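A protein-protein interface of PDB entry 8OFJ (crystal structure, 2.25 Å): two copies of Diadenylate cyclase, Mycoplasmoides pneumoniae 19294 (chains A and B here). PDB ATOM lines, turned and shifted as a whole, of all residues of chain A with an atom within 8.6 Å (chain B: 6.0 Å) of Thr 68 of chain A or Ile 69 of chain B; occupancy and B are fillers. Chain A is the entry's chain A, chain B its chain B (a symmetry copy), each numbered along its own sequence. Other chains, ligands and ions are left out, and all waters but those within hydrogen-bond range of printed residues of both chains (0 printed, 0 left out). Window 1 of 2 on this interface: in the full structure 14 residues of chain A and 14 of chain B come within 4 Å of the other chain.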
ATOM      1  N   ARG A  29      -3.089  16.071  -3.961  1.00  0.00           N
ATOM      2  CA  ARG A  29      -3.055  16.008  -2.508  1.00  0.00           C
ATOM      3  C   ARG A  29      -2.272  17.188  -1.926  1.00  0.00           C
ATOM      4  O   ARG A  29      -2.743  17.855  -1.005  1.00  0.00           O
ATOM      5  CB  ARG A  29      -2.459  14.668  -2.074  1.00  0.00           C
ATOM      6  CG  ARG A  29      -2.347  14.475  -0.570  1.00  0.00           C
ATOM      7  CD  ARG A  29      -1.812  13.096  -0.238  1.00  0.00           C
ATOM      8  NE  ARG A  29      -2.634  12.078  -0.866  1.00  0.00           N
ATOM      9  CZ  ARG A  29      -3.697  11.515  -0.299  1.00  0.00           C
ATOM     10  NH1 ARG A  29      -4.099  11.907   0.896  1.00  0.00           N
ATOM     11  NH2 ARG A  29      -4.359  10.564  -0.931  1.00  0.00           N
ATOM     12  N   LEU A  30      -1.060  17.427  -2.442  1.00  0.00           N
ATOM     13  CA  LEU A  30      -0.214  18.516  -1.976  1.00  0.00           C
ATOM     14  C   LEU A  30      -0.903  19.852  -2.230  1.00  0.00           C
ATOM     15  O   LEU A  30      -0.765  20.789  -1.447  1.00  0.00           O
ATOM     16  CB  LEU A  30       1.126  18.452  -2.711  1.00  0.00           C
ATOM     17  CG  LEU A  30       1.944  17.185  -2.475  1.00  0.00           C
ATOM     18  CD1 LEU A  30       3.046  17.043  -3.501  1.00  0.00           C
ATOM     19  CD2 LEU A  30       2.516  17.175  -1.072  1.00  0.00           C
ATOM     20  N   VAL A  57      17.751   8.495  -2.496  1.00  0.00           N
ATOM     21  CA  VAL A  57      16.767   7.520  -2.086  1.00  0.00           C
ATOM     22  C   VAL A  57      16.191   6.938  -3.370  1.00  0.00           C
ATOM     23  O   VAL A  57      15.738   7.692  -4.228  1.00  0.00           O
ATOM     24  CB  VAL A  57      15.698   8.155  -1.179  1.00  0.00           C
ATOM     25  CG1 VAL A  57      14.871   9.191  -1.907  1.00  0.00           C
ATOM     26  CG2 VAL A  57      14.781   7.117  -0.574  1.00  0.00           C
ATOM     27  N   SER A  62       5.710   6.270  -5.342  1.00  0.00           N
ATOM     28  CA  SER A  62       4.517   5.862  -4.615  1.00  0.00           C
ATOM     29  C   SER A  62       3.976   7.052  -3.829  1.00  0.00           C
ATOM     30  O   SER A  62       4.722   7.723  -3.111  1.00  0.00           O
ATOM     31  CB  SER A  62       4.788   4.689  -3.696  1.00  0.00           C
ATOM     32  OG  SER A  62       5.293   5.131  -2.446  1.00  0.00           O
ATOM     33  N   PRO A  63       2.661   7.342  -3.938  1.00  0.00           N
ATOM     34  CA  PRO A  63       2.038   8.392  -3.136  1.00  0.00           C
ATOM     35  C   PRO A  63       2.304   8.215  -1.644  1.00  0.00           C
ATOM     36  O   PRO A  63       2.461   9.197  -0.920  1.00  0.00           O
ATOM     37  CB  PRO A  63       0.541   8.237  -3.448  1.00  0.00           C
ATOM     38  CG  PRO A  63       0.522   7.620  -4.828  1.00  0.00           C
ATOM     39  CD  PRO A  63       1.707   6.678  -4.841  1.00  0.00           C
ATOM     40  N   GLU A  64       2.382   6.947  -1.212  1.00  0.00           N
ATOM     41  CA  GLU A  64       2.619   6.595   0.182  1.00  0.00           C
ATOM     42  C   GLU A  64       3.975   7.130   0.640  1.00  0.00           C
ATOM     43  O   GLU A  64       4.083   7.718   1.712  1.00  0.00           O
ATOM     44  CB  GLU A  64       2.580   5.080   0.392  1.00  0.00           C
ATOM     45  CG  GLU A  64       1.231   4.453   0.085  1.00  0.00           C
ATOM     46  CD  GLU A  64       0.905   4.216  -1.382  1.00  0.00           C
ATOM     47  OE1 GLU A  64       1.821   4.343  -2.233  1.00  0.00           O
ATOM     48  OE2 GLU A  64      -0.276   3.921  -1.673  1.00  0.00           O
ATOM     49  N   LEU A  65       5.009   6.938  -0.175  1.00  0.00           N
ATOM     50  CA  LEU A  65       6.329   7.421   0.187  1.00  0.00           C
ATOM     51  C   LEU A  65       6.351   8.947   0.128  1.00  0.00           C
ATOM     52  O   LEU A  65       6.849   9.588   1.041  1.00  0.00           O
ATOM     53  CB  LEU A  65       7.378   6.783  -0.728  1.00  0.00           C
ATOM     54  CG  LEU A  65       8.821   7.233  -0.505  1.00  0.00           C
ATOM     55  CD1 LEU A  65       9.310   6.891   0.894  1.00  0.00           C
ATOM     56  CD2 LEU A  65       9.742   6.610  -1.542  1.00  0.00           C
ATOM     57  N   LEU A  66       5.761   9.543  -0.910  1.00  0.00           N
ATOM     58  CA  LEU A  66       5.777  10.996  -1.036  1.00  0.00           C
ATOM     59  C   LEU A  66       4.964  11.672   0.066  1.00  0.00           C
ATOM     60  O   LEU A  66       5.278  12.787   0.463  1.00  0.00           O
ATOM     61  CB  LEU A  66       5.290  11.412  -2.426  1.00  0.00           C
ATOM     62  CG  LEU A  66       6.415  11.824  -3.374  1.00  0.00           C
ATOM     63  CD1 LEU A  66       7.264  10.636  -3.777  1.00  0.00           C
ATOM     64  CD2 LEU A  66       5.859  12.500  -4.603  1.00  0.00           C
ATOM     65  N   VAL A  67       3.933  11.001   0.584  1.00  0.00           N
ATOM     66  CA  VAL A  67       3.239  11.503   1.760  1.00  0.00           C
ATOM     67  C   VAL A  67       4.185  11.453   2.966  1.00  0.00           C
ATOM     68  O   VAL A  67       4.318  12.438   3.684  1.00  0.00           O
ATOM     69  CB  VAL A  67       1.923  10.735   2.001  1.00  0.00           C
ATOM     70  CG1 VAL A  67       1.421  10.841   3.440  1.00  0.00           C
ATOM     71  CG2 VAL A  67       0.848  11.182   1.029  1.00  0.00           C
ATOM     72  N   THR A  68       4.855  10.316   3.184  1.00  0.00           N
ATOM     73  CA  THR A  68       5.764  10.193   4.314  1.00  0.00           C
ATOM     74  C   THR A  68       6.728  11.379   4.342  1.00  0.00           C
ATOM     75  O   THR A  68       6.901  11.999   5.388  1.00  0.00           O
ATOM     76  CB  THR A  68       6.540   8.868   4.309  1.00  0.00           C
ATOM     77  OG1 THR A  68       5.639   7.756   4.265  1.00  0.00           O
ATOM     78  CG2 THR A  68       7.420   8.719   5.528  1.00  0.00           C
ATOM     79  N   ILE A  69       7.339  11.681   3.193  1.00  0.00           N
ATOM     80  CA  ILE A  69       8.313  12.756   3.055  1.00  0.00           C
ATOM     81  C   ILE A  69       7.672  14.111   3.361  1.00  0.00           C
ATOM     82  O   ILE A  69       8.140  14.836   4.243  1.00  0.00           O
ATOM     83  CB  ILE A  69       8.935  12.721   1.640  1.00  0.00           C
ATOM     84  CG1 ILE A  69       9.998  11.627   1.529  1.00  0.00           C
ATOM     85  CG2 ILE A  69       9.494  14.077   1.226  1.00  0.00           C
ATOM     86  CD1 ILE A  69      10.403  11.299   0.104  1.00  0.00           C
ATOM     87  N   PHE A  70       6.616  14.462   2.618  1.00  0.00           N
ATOM     88  CA  PHE A  70       6.180  15.852   2.525  1.00  0.00           C
ATOM     89  C   PHE A  70       5.286  16.264   3.693  1.00  0.00           C
ATOM     90  O   PHE A  70       5.191  17.454   3.965  1.00  0.00           O
ATOM     91  CB  PHE A  70       5.440  16.110   1.211  1.00  0.00           C
ATOM     92  CG  PHE A  70       6.325  16.392   0.024  1.00  0.00           C
ATOM     93  CD1 PHE A  70       7.077  17.556  -0.042  1.00  0.00           C
ATOM     94  CD2 PHE A  70       6.382  15.514  -1.049  1.00  0.00           C
ATOM     95  CE1 PHE A  70       7.886  17.819  -1.138  1.00  0.00           C
ATOM     96  CE2 PHE A  70       7.177  15.790  -2.152  1.00  0.00           C
ATOM     97  CZ  PHE A  70       7.930  16.939  -2.193  1.00  0.00           C
ATOM     98  N   TYR A  71       4.642  15.297   4.367  1.00  0.00           N
ATOM     99  CA  TYR A  71       3.741  15.594   5.476  1.00  0.00           C
ATOM    100  C   TYR A  71       4.487  15.578   6.809  1.00  0.00           C
ATOM    101  O   TYR A  71       3.913  15.223   7.836  1.00  0.00           O
ATOM    102  CB  TYR A  71       2.556  14.624   5.497  1.00  0.00           C
ATOM    103  CG  TYR A  71       1.427  15.024   4.583  1.00  0.00           C
ATOM    104  CD1 TYR A  71       1.581  15.012   3.204  1.00  0.00           C
ATOM    105  CD2 TYR A  71       0.207  15.440   5.095  1.00  0.00           C
ATOM    106  CE1 TYR A  71       0.551  15.395   2.359  1.00  0.00           C
ATOM    107  CE2 TYR A  71      -0.835  15.819   4.265  1.00  0.00           C
ATOM    108  CZ  TYR A  71      -0.662  15.796   2.892  1.00  0.00           C
ATOM    109  OH  TYR A  71      -1.681  16.155   2.046  1.00  0.00           O
ATOM    110  N   ASN A  72       5.755  15.994   6.786  1.00  0.00           N
ATOM    111  CA  ASN A  72       6.549  16.159   7.990  1.00  0.00           C
ATOM    112  C   ASN A  72       7.386  17.423   7.800  1.00  0.00           C
ATOM    113  O   ASN A  72       8.447  17.392   7.176  1.00  0.00           O
ATOM    114  CB  ASN A  72       7.371  14.897   8.276  1.00  0.00           C
ATOM    115  CG  ASN A  72       8.075  14.921   9.619  1.00  0.00           C
ATOM    116  OD1 ASN A  72       9.298  14.804   9.681  1.00  0.00           O
ATOM    117  ND2 ASN A  72       7.316  15.047  10.696  1.00  0.00           N
ATOM    118  N   LYS A  73       6.856  18.545   8.302  1.00  0.00           N
ATOM    119  CA  LYS A  73       7.445  19.861   8.097  1.00  0.00           C
ATOM    120  C   LYS A  73       8.756  20.007   8.873  1.00  0.00           C
ATOM    121  O   LYS A  73       9.517  20.939   8.609  1.00  0.00           O
ATOM    122  CB  LYS A  73       6.462  20.958   8.525  1.00  0.00           C
ATOM    123  CG  LYS A  73       6.117  20.975  10.012  1.00  0.00           C
ATOM    124  CD  LYS A  73       4.934  21.853  10.378  1.00  0.00           C
ATOM    125  CE  LYS A  73       4.512  21.676  11.824  1.00  0.00           C
ATOM    126  NZ  LYS A  73       3.189  22.277  12.110  1.00  0.00           N
ATOM    127  N   SER A  75      11.071  17.552   8.983  1.00  0.00           N
ATOM    128  CA  SER A  75      12.069  16.775   8.258  1.00  0.00           C
ATOM    129  C   SER A  75      12.670  17.598   7.116  1.00  0.00           C
ATOM    130  O   SER A  75      11.945  18.309   6.420  1.00  0.00           O
ATOM    131  CB  SER A  75      11.469  15.464   7.762  1.00  0.00           C
ATOM    132  OG  SER A  75      12.152  14.961   6.623  1.00  0.00           O
ATOM    133  N   LEU A  77      13.742  16.362   4.392  1.00  0.00           N
ATOM    134  CA  LEU A  77      13.352  15.667   3.171  1.00  0.00           C
ATOM    135  C   LEU A  77      12.185  16.397   2.501  1.00  0.00           C
ATOM    136  O   LEU A  77      12.087  16.390   1.275  1.00  0.00           O
ATOM    137  CB  LEU A  77      13.001  14.212   3.506  1.00  0.00           C
ATOM    138  CG  LEU A  77      14.085  13.416   4.240  1.00  0.00           C
ATOM    139  CD1 LEU A  77      13.792  11.926   4.166  1.00  0.00           C
ATOM    140  CD2 LEU A  77      15.479  13.717   3.694  1.00  0.00           C
ATOM    141  N   HIS A  78      11.350  17.077   3.307  1.00  0.00           N
ATOM    142  CA  HIS A  78      10.223  17.850   2.798  1.00  0.00           C
ATOM    143  C   HIS A  78      10.712  19.098   2.060  1.00  0.00           C
ATOM    144  O   HIS A  78       9.948  19.719   1.322  1.00  0.00           O
ATOM    145  CB  HIS A  78       9.224  18.189   3.918  1.00  0.00           C
ATOM    146  CG  HIS A  78       9.331  19.566   4.491  1.00  0.00           C
ATOM    147  ND1 HIS A  78      10.261  19.964   5.428  1.00  0.00           N
ATOM    148  CD2 HIS A  78       8.560  20.636   4.265  1.00  0.00           C
ATOM    149  CE1 HIS A  78      10.065  21.242   5.730  1.00  0.00           C
ATOM    150  NE2 HIS A  78       9.035  21.670   5.034  1.00  0.00           N
ATOM    151  N   GLU B  64      16.656  10.537  10.683  1.00  0.00           N
ATOM    152  CA  GLU B  64      15.567  11.425  10.306  1.00  0.00           C
ATOM    153  C   GLU B  64      14.526  10.677   9.480  1.00  0.00           C
ATOM    154  O   GLU B  64      13.339  10.759   9.750  1.00  0.00           O
ATOM    155  CB  GLU B  64      16.078  12.631   9.513  1.00  0.00           C
ATOM    156  CG  GLU B  64      16.292  13.877  10.364  1.00  0.00           C
ATOM    157  CD  GLU B  64      15.014  14.457  10.953  1.00  0.00           C
ATOM    158  OE1 GLU B  64      14.029  14.617  10.191  1.00  0.00           O
ATOM    159  OE2 GLU B  64      15.005  14.755  12.174  1.00  0.00           O
ATOM    160  N   LEU B  65      14.992   9.946   8.472  1.00  0.00           N
ATOM    161  CA  LEU B  65      14.113   9.221   7.578  1.00  0.00           C
ATOM    162  C   LEU B  65      13.389   8.091   8.317  1.00  0.00           C
ATOM    163  O   LEU B  65      12.187   7.931   8.154  1.00  0.00           O
ATOM    164  CB  LEU B  65      14.966   8.701   6.420  1.00  0.00           C
ATOM    165  CG  LEU B  65      14.266   7.750   5.456  1.00  0.00           C
ATOM    166  CD1 LEU B  65      12.995   8.368   4.884  1.00  0.00           C
ATOM    167  CD2 LEU B  65      15.212   7.361   4.334  1.00  0.00           C
ATOM    168  N   LEU B  66      14.103   7.333   9.157  1.00  0.00           N
ATOM    169  CA  LEU B  66      13.491   6.288   9.974  1.00  0.00           C
ATOM    170  C   LEU B  66      12.343   6.834  10.833  1.00  0.00           C
ATOM    171  O   LEU B  66      11.306   6.184  10.984  1.00  0.00           O
ATOM    172  CB  LEU B  66      14.555   5.637  10.870  1.00  0.00           C
ATOM    173  CG  LEU B  66      15.335   4.472  10.270  1.00  0.00           C
ATOM    174  CD1 LEU B  66      14.419   3.422   9.653  1.00  0.00           C
ATOM    175  CD2 LEU B  66      16.322   4.976   9.247  1.00  0.00           C
ATOM    176  N   VAL B  67      12.526   8.036  11.388  1.00  0.00           N
ATOM    177  CA  VAL B  67      11.523   8.645  12.245  1.00  0.00           C
ATOM    178  C   VAL B  67      10.312   9.072  11.424  1.00  0.00           C
ATOM    179  O   VAL B  67       9.189   8.863  11.861  1.00  0.00           O
ATOM    180  CB  VAL B  67      12.118   9.803  13.069  1.00  0.00           C
ATOM    181  CG1 VAL B  67      11.060  10.772  13.578  1.00  0.00           C
ATOM    182  CG2 VAL B  67      12.949   9.263  14.226  1.00  0.00           C
ATOM    183  N   THR B  68      10.518   9.657  10.238  1.00  0.00           N
ATOM    184  CA  THR B  68       9.375  10.080   9.438  1.00  0.00           C
ATOM    185  C   THR B  68       8.574   8.850   8.983  1.00  0.00           C
ATOM    186  O   THR B  68       7.357   8.921   8.892  1.00  0.00           O
ATOM    187  CB  THR B  68       9.758  11.009   8.276  1.00  0.00           C
ATOM    188  OG1 THR B  68      10.066  10.241   7.112  1.00  0.00           O
ATOM    189  CG2 THR B  68      10.903  11.947   8.598  1.00  0.00           C
ATOM    190  N   ILE B  69       9.241   7.706   8.748  1.00  0.00           N
ATOM    191  CA  ILE B  69       8.551   6.482   8.359  1.00  0.00           C
ATOM    192  C   ILE B  69       7.600   6.006   9.462  1.00  0.00           C
ATOM    193  O   ILE B  69       6.431   5.759   9.207  1.00  0.00           O
ATOM    194  CB  ILE B  69       9.563   5.386   7.971  1.00  0.00           C
ATOM    195  CG1 ILE B  69      10.279   5.745   6.674  1.00  0.00           C
ATOM    196  CG2 ILE B  69       8.903   4.021   7.885  1.00  0.00           C
ATOM    197  CD1 ILE B  69      11.503   4.901   6.388  1.00  0.00           C
ATOM    198  N   PHE B  70       8.080   5.845  10.687  1.00  0.00           N
ATOM    199  CA  PHE B  70       7.275   5.189  11.711  1.00  0.00           C
ATOM    200  C   PHE B  70       6.310   6.164  12.392  1.00  0.00           C
ATOM    201  O   PHE B  70       5.250   5.753  12.876  1.00  0.00           O
ATOM    202  CB  PHE B  70       8.180   4.476  12.716  1.00  0.00           C
ATOM    203  CG  PHE B  70       8.817   3.233  12.156  1.00  0.00           C
ATOM    204  CD1 PHE B  70       8.035   2.181  11.722  1.00  0.00           C
ATOM    205  CD2 PHE B  70      10.196   3.122  12.049  1.00  0.00           C
ATOM    206  CE1 PHE B  70       8.614   1.031  11.213  1.00  0.00           C
ATOM    207  CE2 PHE B  70      10.773   1.965  11.561  1.00  0.00           C
ATOM    208  CZ  PHE B  70       9.980   0.930  11.125  1.00  0.00           C
ATOM    209  N   TYR B  71       6.683   7.445  12.431  1.00  0.00           N
ATOM    210  CA  TYR B  71       5.874   8.446  13.101  1.00  0.00           C
ATOM    211  C   TYR B  71       4.680   8.845  12.240  1.00  0.00           C
ATOM    212  O   TYR B  71       3.608   9.115  12.762  1.00  0.00           O
ATOM    213  CB  TYR B  71       6.712   9.680  13.433  1.00  0.00           C
ATOM    214  CG  TYR B  71       5.925  10.807  14.055  1.00  0.00           C
ATOM    215  CD1 TYR B  71       5.543  10.775  15.392  1.00  0.00           C
ATOM    216  CD2 TYR B  71       5.511  11.884  13.282  1.00  0.00           C
ATOM    217  CE1 TYR B  71       4.799  11.805  15.951  1.00  0.00           C
ATOM    218  CE2 TYR B  71       4.769  12.922  13.826  1.00  0.00           C
ATOM    219  CZ  TYR B  71       4.413  12.881  15.165  1.00  0.00           C
ATOM    220  OH  TYR B  71       3.683  13.907  15.706  1.00  0.00           O
ATOM    221  N   ASN B  72       4.872   8.895  10.921  1.00  0.00           N
ATOM    222  CA  ASN B  72       3.842   9.390  10.031  1.00  0.00           C
ATOM    223  C   ASN B  72       2.700   8.372   9.978  1.00  0.00           C
ATOM    224  O   ASN B  72       2.804   7.353   9.300  1.00  0.00           O
ATOM    225  CB  ASN B  72       4.421   9.713   8.656  1.00  0.00           C
ATOM    226  CG  ASN B  72       3.510  10.591   7.821  1.00  0.00           C
ATOM    227  OD1 ASN B  72       2.291  10.407   7.841  1.00  0.00           O
ATOM    228  ND2 ASN B  72       4.084  11.544   7.097  1.00  0.00           N
ATOM    229  N   LYS B  73       1.594   8.682  10.671  1.00  0.00           N
ATOM    230  CA  LYS B  73       0.459   7.772  10.806  1.00  0.00           C
ATOM    231  C   LYS B  73      -0.461   7.789   9.579  1.00  0.00           C
ATOM    232  O   LYS B  73      -1.246   6.865   9.394  1.00  0.00           O
ATOM    233  CB  LYS B  73      -0.371   8.112  12.052  1.00  0.00           C
ATOM    234  CG  LYS B  73       0.214   7.665  13.387  1.00  0.00           C
ATOM    235  CD  LYS B  73       0.699   6.230  13.393  1.00  0.00           C
ATOM    236  CE  LYS B  73       0.883   5.656  14.783  1.00  0.00           C
ATOM    237  NZ  LYS B  73       1.900   6.404  15.564  1.00  0.00           N
ATOM    238  N   SER B  75       0.418   7.620   6.372  1.00  0.00           N
ATOM    239  CA  SER B  75       0.910   6.683   5.372  1.00  0.00           C
ATOM    240  C   SER B  75       0.950   5.271   5.950  1.00  0.00           C
ATOM    241  O   SER B  75       1.321   5.098   7.107  1.00  0.00           O
ATOM    242  CB  SER B  75       2.277   7.114   4.892  1.00  0.00           C
ATOM    243  OG  SER B  75       2.768   6.258   3.867  1.00  0.00           O
ATOM    244  N   LEU B  77       3.194   3.213   5.414  1.00  0.00           N
ATOM    245  CA  LEU B  77       4.605   2.894   5.551  1.00  0.00           C
ATOM    246  C   LEU B  77       4.981   2.687   7.018  1.00  0.00           C
ATOM    247  O   LEU B  77       5.947   1.988   7.307  1.00  0.00           O
ATOM    248  CB  LEU B  77       5.450   4.021   4.944  1.00  0.00           C
ATOM    249  CG  LEU B  77       5.418   4.190   3.419  1.00  0.00           C
ATOM    250  CD1 LEU B  77       6.758   4.691   2.923  1.00  0.00           C
ATOM    251  CD2 LEU B  77       5.041   2.915   2.684  1.00  0.00           C
ATOM    252  N   HIS B  78       4.226   3.280   7.947  1.00  0.00           N
ATOM    253  CA  HIS B  78       4.557   3.188   9.358  1.00  0.00           C
ATOM    254  C   HIS B  78       4.293   1.782   9.897  1.00  0.00           C
ATOM    255  O   HIS B  78       4.736   1.452  10.988  1.00  0.00           O
ATOM    256  CB  HIS B  78       3.761   4.214  10.171  1.00  0.00           C
ATOM    257  CG  HIS B  78       2.375   3.790  10.501  1.00  0.00           C
ATOM    258  ND1 HIS B  78       1.310   3.974   9.650  1.00  0.00           N
ATOM    259  CD2 HIS B  78       1.882   3.215  11.605  1.00  0.00           C
ATOM    260  CE1 HIS B  78       0.209   3.512  10.228  1.00  0.00           C
ATOM    261  NE2 HIS B  78       0.537   3.039  11.412  1.00  0.00           N
ATOM    262  N   ASP B  79       3.508   0.986   9.169  1.00  0.00           N
ATOM    263  CA  ASP B  79       3.190  -0.368   9.583  1.00  0.00           C
ATOM    264  C   ASP B  79       4.177  -1.331   8.925  1.00  0.00           C
ATOM    265  O   ASP B  79       4.640  -1.117   7.802  1.00  0.00           O
ATOM    266  CB  ASP B  79       1.753  -0.743   9.195  1.00  0.00           C
ATOM    267  CG  ASP B  79       0.677  -0.245  10.146  1.00  0.00           C
ATOM    268  OD1 ASP B  79       1.012   0.109  11.304  1.00  0.00           O
ATOM    269  OD2 ASP B  79      -0.497  -0.188   9.707  1.00  0.00           O
ATOM    270  N   VAL B  82      10.924  -2.257   8.565  1.00  0.00           N
ATOM    271  CA  VAL B  82      12.059  -1.834   7.774  1.00  0.00           C
ATOM    272  C   VAL B  82      13.101  -2.955   7.763  1.00  0.00           C
ATOM    273  O   VAL B  82      13.467  -3.507   8.803  1.00  0.00           O
ATOM    274  CB  VAL B  82      12.631  -0.518   8.336  1.00  0.00           C
ATOM    275  CG1 VAL B  82      13.979  -0.151   7.735  1.00  0.00           C
ATOM    276  CG2 VAL B  82      11.649   0.635   8.179  1.00  0.00           C
ATOM    277  N   ILE B  89      18.993   0.777   4.285  1.00  0.00           N
ATOM    278  CA  ILE B  89      17.596   0.414   4.162  1.00  0.00           C
ATOM    279  C   ILE B  89      17.351  -0.164   2.772  1.00  0.00           C
ATOM    280  O   ILE B  89      17.757   0.441   1.778  1.00  0.00           O
ATOM    281  CB  ILE B  89      16.710   1.645   4.384  1.00  0.00           C
ATOM    282  CG1 ILE B  89      16.879   2.206   5.798  1.00  0.00           C
ATOM    283  CG2 ILE B  89      15.262   1.315   4.064  1.00  0.00           C
ATOM    284  CD1 ILE B  89      16.307   3.603   5.978  1.00  0.00           C
ATOM    285  N   VAL B  92      10.646  -1.055   3.212  1.00  0.00           N
ATOM    286  CA  VAL B  92       9.783  -0.643   4.312  1.00  0.00           C
ATOM    287  C   VAL B  92       8.453  -1.382   4.165  1.00  0.00           C
ATOM    288  O   VAL B  92       8.161  -1.930   3.105  1.00  0.00           O
ATOM    289  CB  VAL B  92       9.582   0.889   4.339  1.00  0.00           C
ATOM    290  CG1 VAL B  92      10.907   1.642   4.254  1.00  0.00           C
ATOM    291  CG2 VAL B  92       8.669   1.355   3.230  1.00  0.00           C
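O of Thr 68 of chain A is in hydrogen-bond range of ND2 of Asn 72 of chain B.
The side-chain hydroxyl (OG1) of Thr 68 of chain A lies within hydrogen-bond range of the side-chain hydroxyl (OG) of Ser 75 of chain B (3.3 Å).
The backbone carbonyl oxygen of Glu 64 of chain A is in hydrogen-bond range of the side-chain hydroxyl of Ser 75 of chain B (2.9 Å).
The side-chain hydroxyl (OG) of Ser 75 of chain B sits close to the backbone NH (N) of Leu 77 of chain B, at 3.4 Å.
The backbone carbonyl oxygen (O) of Ser 75 of chain B sits at hydrogen-bond distance from a ring nitrogen (ND1) of His 78 of chain B.
OG1 of Thr 68 of chain A lies within hydrogen-bond range of O of Glu 64 of chain A (3.0 Å).
The backbone NH (N) of Leu 65 of chain A is in hydrogen-bond range of the side-chain hydroxyl (OG) of Ser 62 of chain A.
N of Ser 75 of chain A sits close to OD1 of Asn 72 of chain A (3.3 Å).
A ring nitrogen (ND1) of His 78 of chain A sits at hydrogen-bond distance from the backbone carbonyl oxygen (O) of Ser 75 of chain A (2.6 Å).
Among the printed residues, merely in contact across the chains: Glu 64 of chain A with Leu 77 of chain B, Leu 65 of chain A with Leu 77 of chain B, Val 67 of chain A with Asn 72 of chain B, Thr 68 of chain A with Thr 68 of chain B, Thr 68 of chain A with Ile 69 of chain B, Thr 68 of chain A with Leu 77 of chain B, Tyr 71 of chain A with Asn 72 of chain B, Asn 72 of chain A with Thr 68 of chain B, Ser 75 of chain A with Glu 64 of chain B, Ser 75 of chain A with Thr 68 of chain B and Leu 77 of chain A with Leu 65 of chain B.
Of chain B, only Thr 68 (3.4 Å), Ile 69 (3.8 Å), Asn 72 (3.3 Å), Ser 75 (3.3 Å) and Leu 77 (3.5 Å) come within 4 Å of Thr 68 of chain A.
Ile 69 of chain B touches just one residue of chain A: Thr 68.
Printed residues of chain B within 4 Å of Val 67 of chain A: Asn 72.
Of the printed residues of chain A, Leu 77 of chain B touches Glu 64 (3.9996 Å), Leu 65 (3.9 Å) and Thr 68 (3.5 Å).
Of the printed residues of chain A, Glu 64 of chain B touches Ser 75 (3.5 Å).
Printed residues of chain B within 4 Å of Ser 75 of chain A: Glu 64 and Thr 68.
His 78 of chain A touches none of the printed residues of chain B.
Arg 29 of chain A touches none of the printed residues of chain B.
The nearest residue of chain B that does not touch Thr 68 of chain A is Leu 65 of chain B (5.5 Å).
The nearest residue of chain A that does not touch Ile 69 of chain B is Leu 65 of chain A (6.0 Å).
The nearest printed residue of chain B that does not touch Tyr 71 of chain A is Tyr 71 of chain B (6.5 Å).
Hydrophobic or aromatic side chains of chain A that line the printed part of chain B: Leu 65, Tyr 71 and Leu 77.
Printed residues of chain B that touch a printed residue of chain A: Glu 64, Leu 65, Thr 68, Ile 69, Asn 72, Ser 75 and Leu 77.
Among the printed residues, no Asp or Glu carboxylate lies within 4 Å of a Lys or Arg side-chain nitrogen of the other chain.
Glu 64 of chain A touches Ser 75 of chain B, and with the chains exchanged Ser 75 of chain A touches Glu 64 of chain B.
Glu 64 of chain A touches Leu 77 of chain B, but with the chains exchanged Leu 77 of chain A does not touch Glu 64 of chain B (5.5 Å).
Leu 65 of chain A touches Leu 77 of chain B, and with the chains exchanged Leu 77 of chain A touches Leu 65 of chain B.
Thr 68 of chain A touches Ser 75 of chain B, and with the chains exchanged Ser 75 of chain A touches Thr 68 of chain B.
Positions printed for both chains: 64, 65, 66, 67, 68, 69, 70, 71, 72, 73, 75, 77 and 78.
Of the 14 pairs that touch across the chains among the printed residues, 9 have their exchanged pair printed and touching as well.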
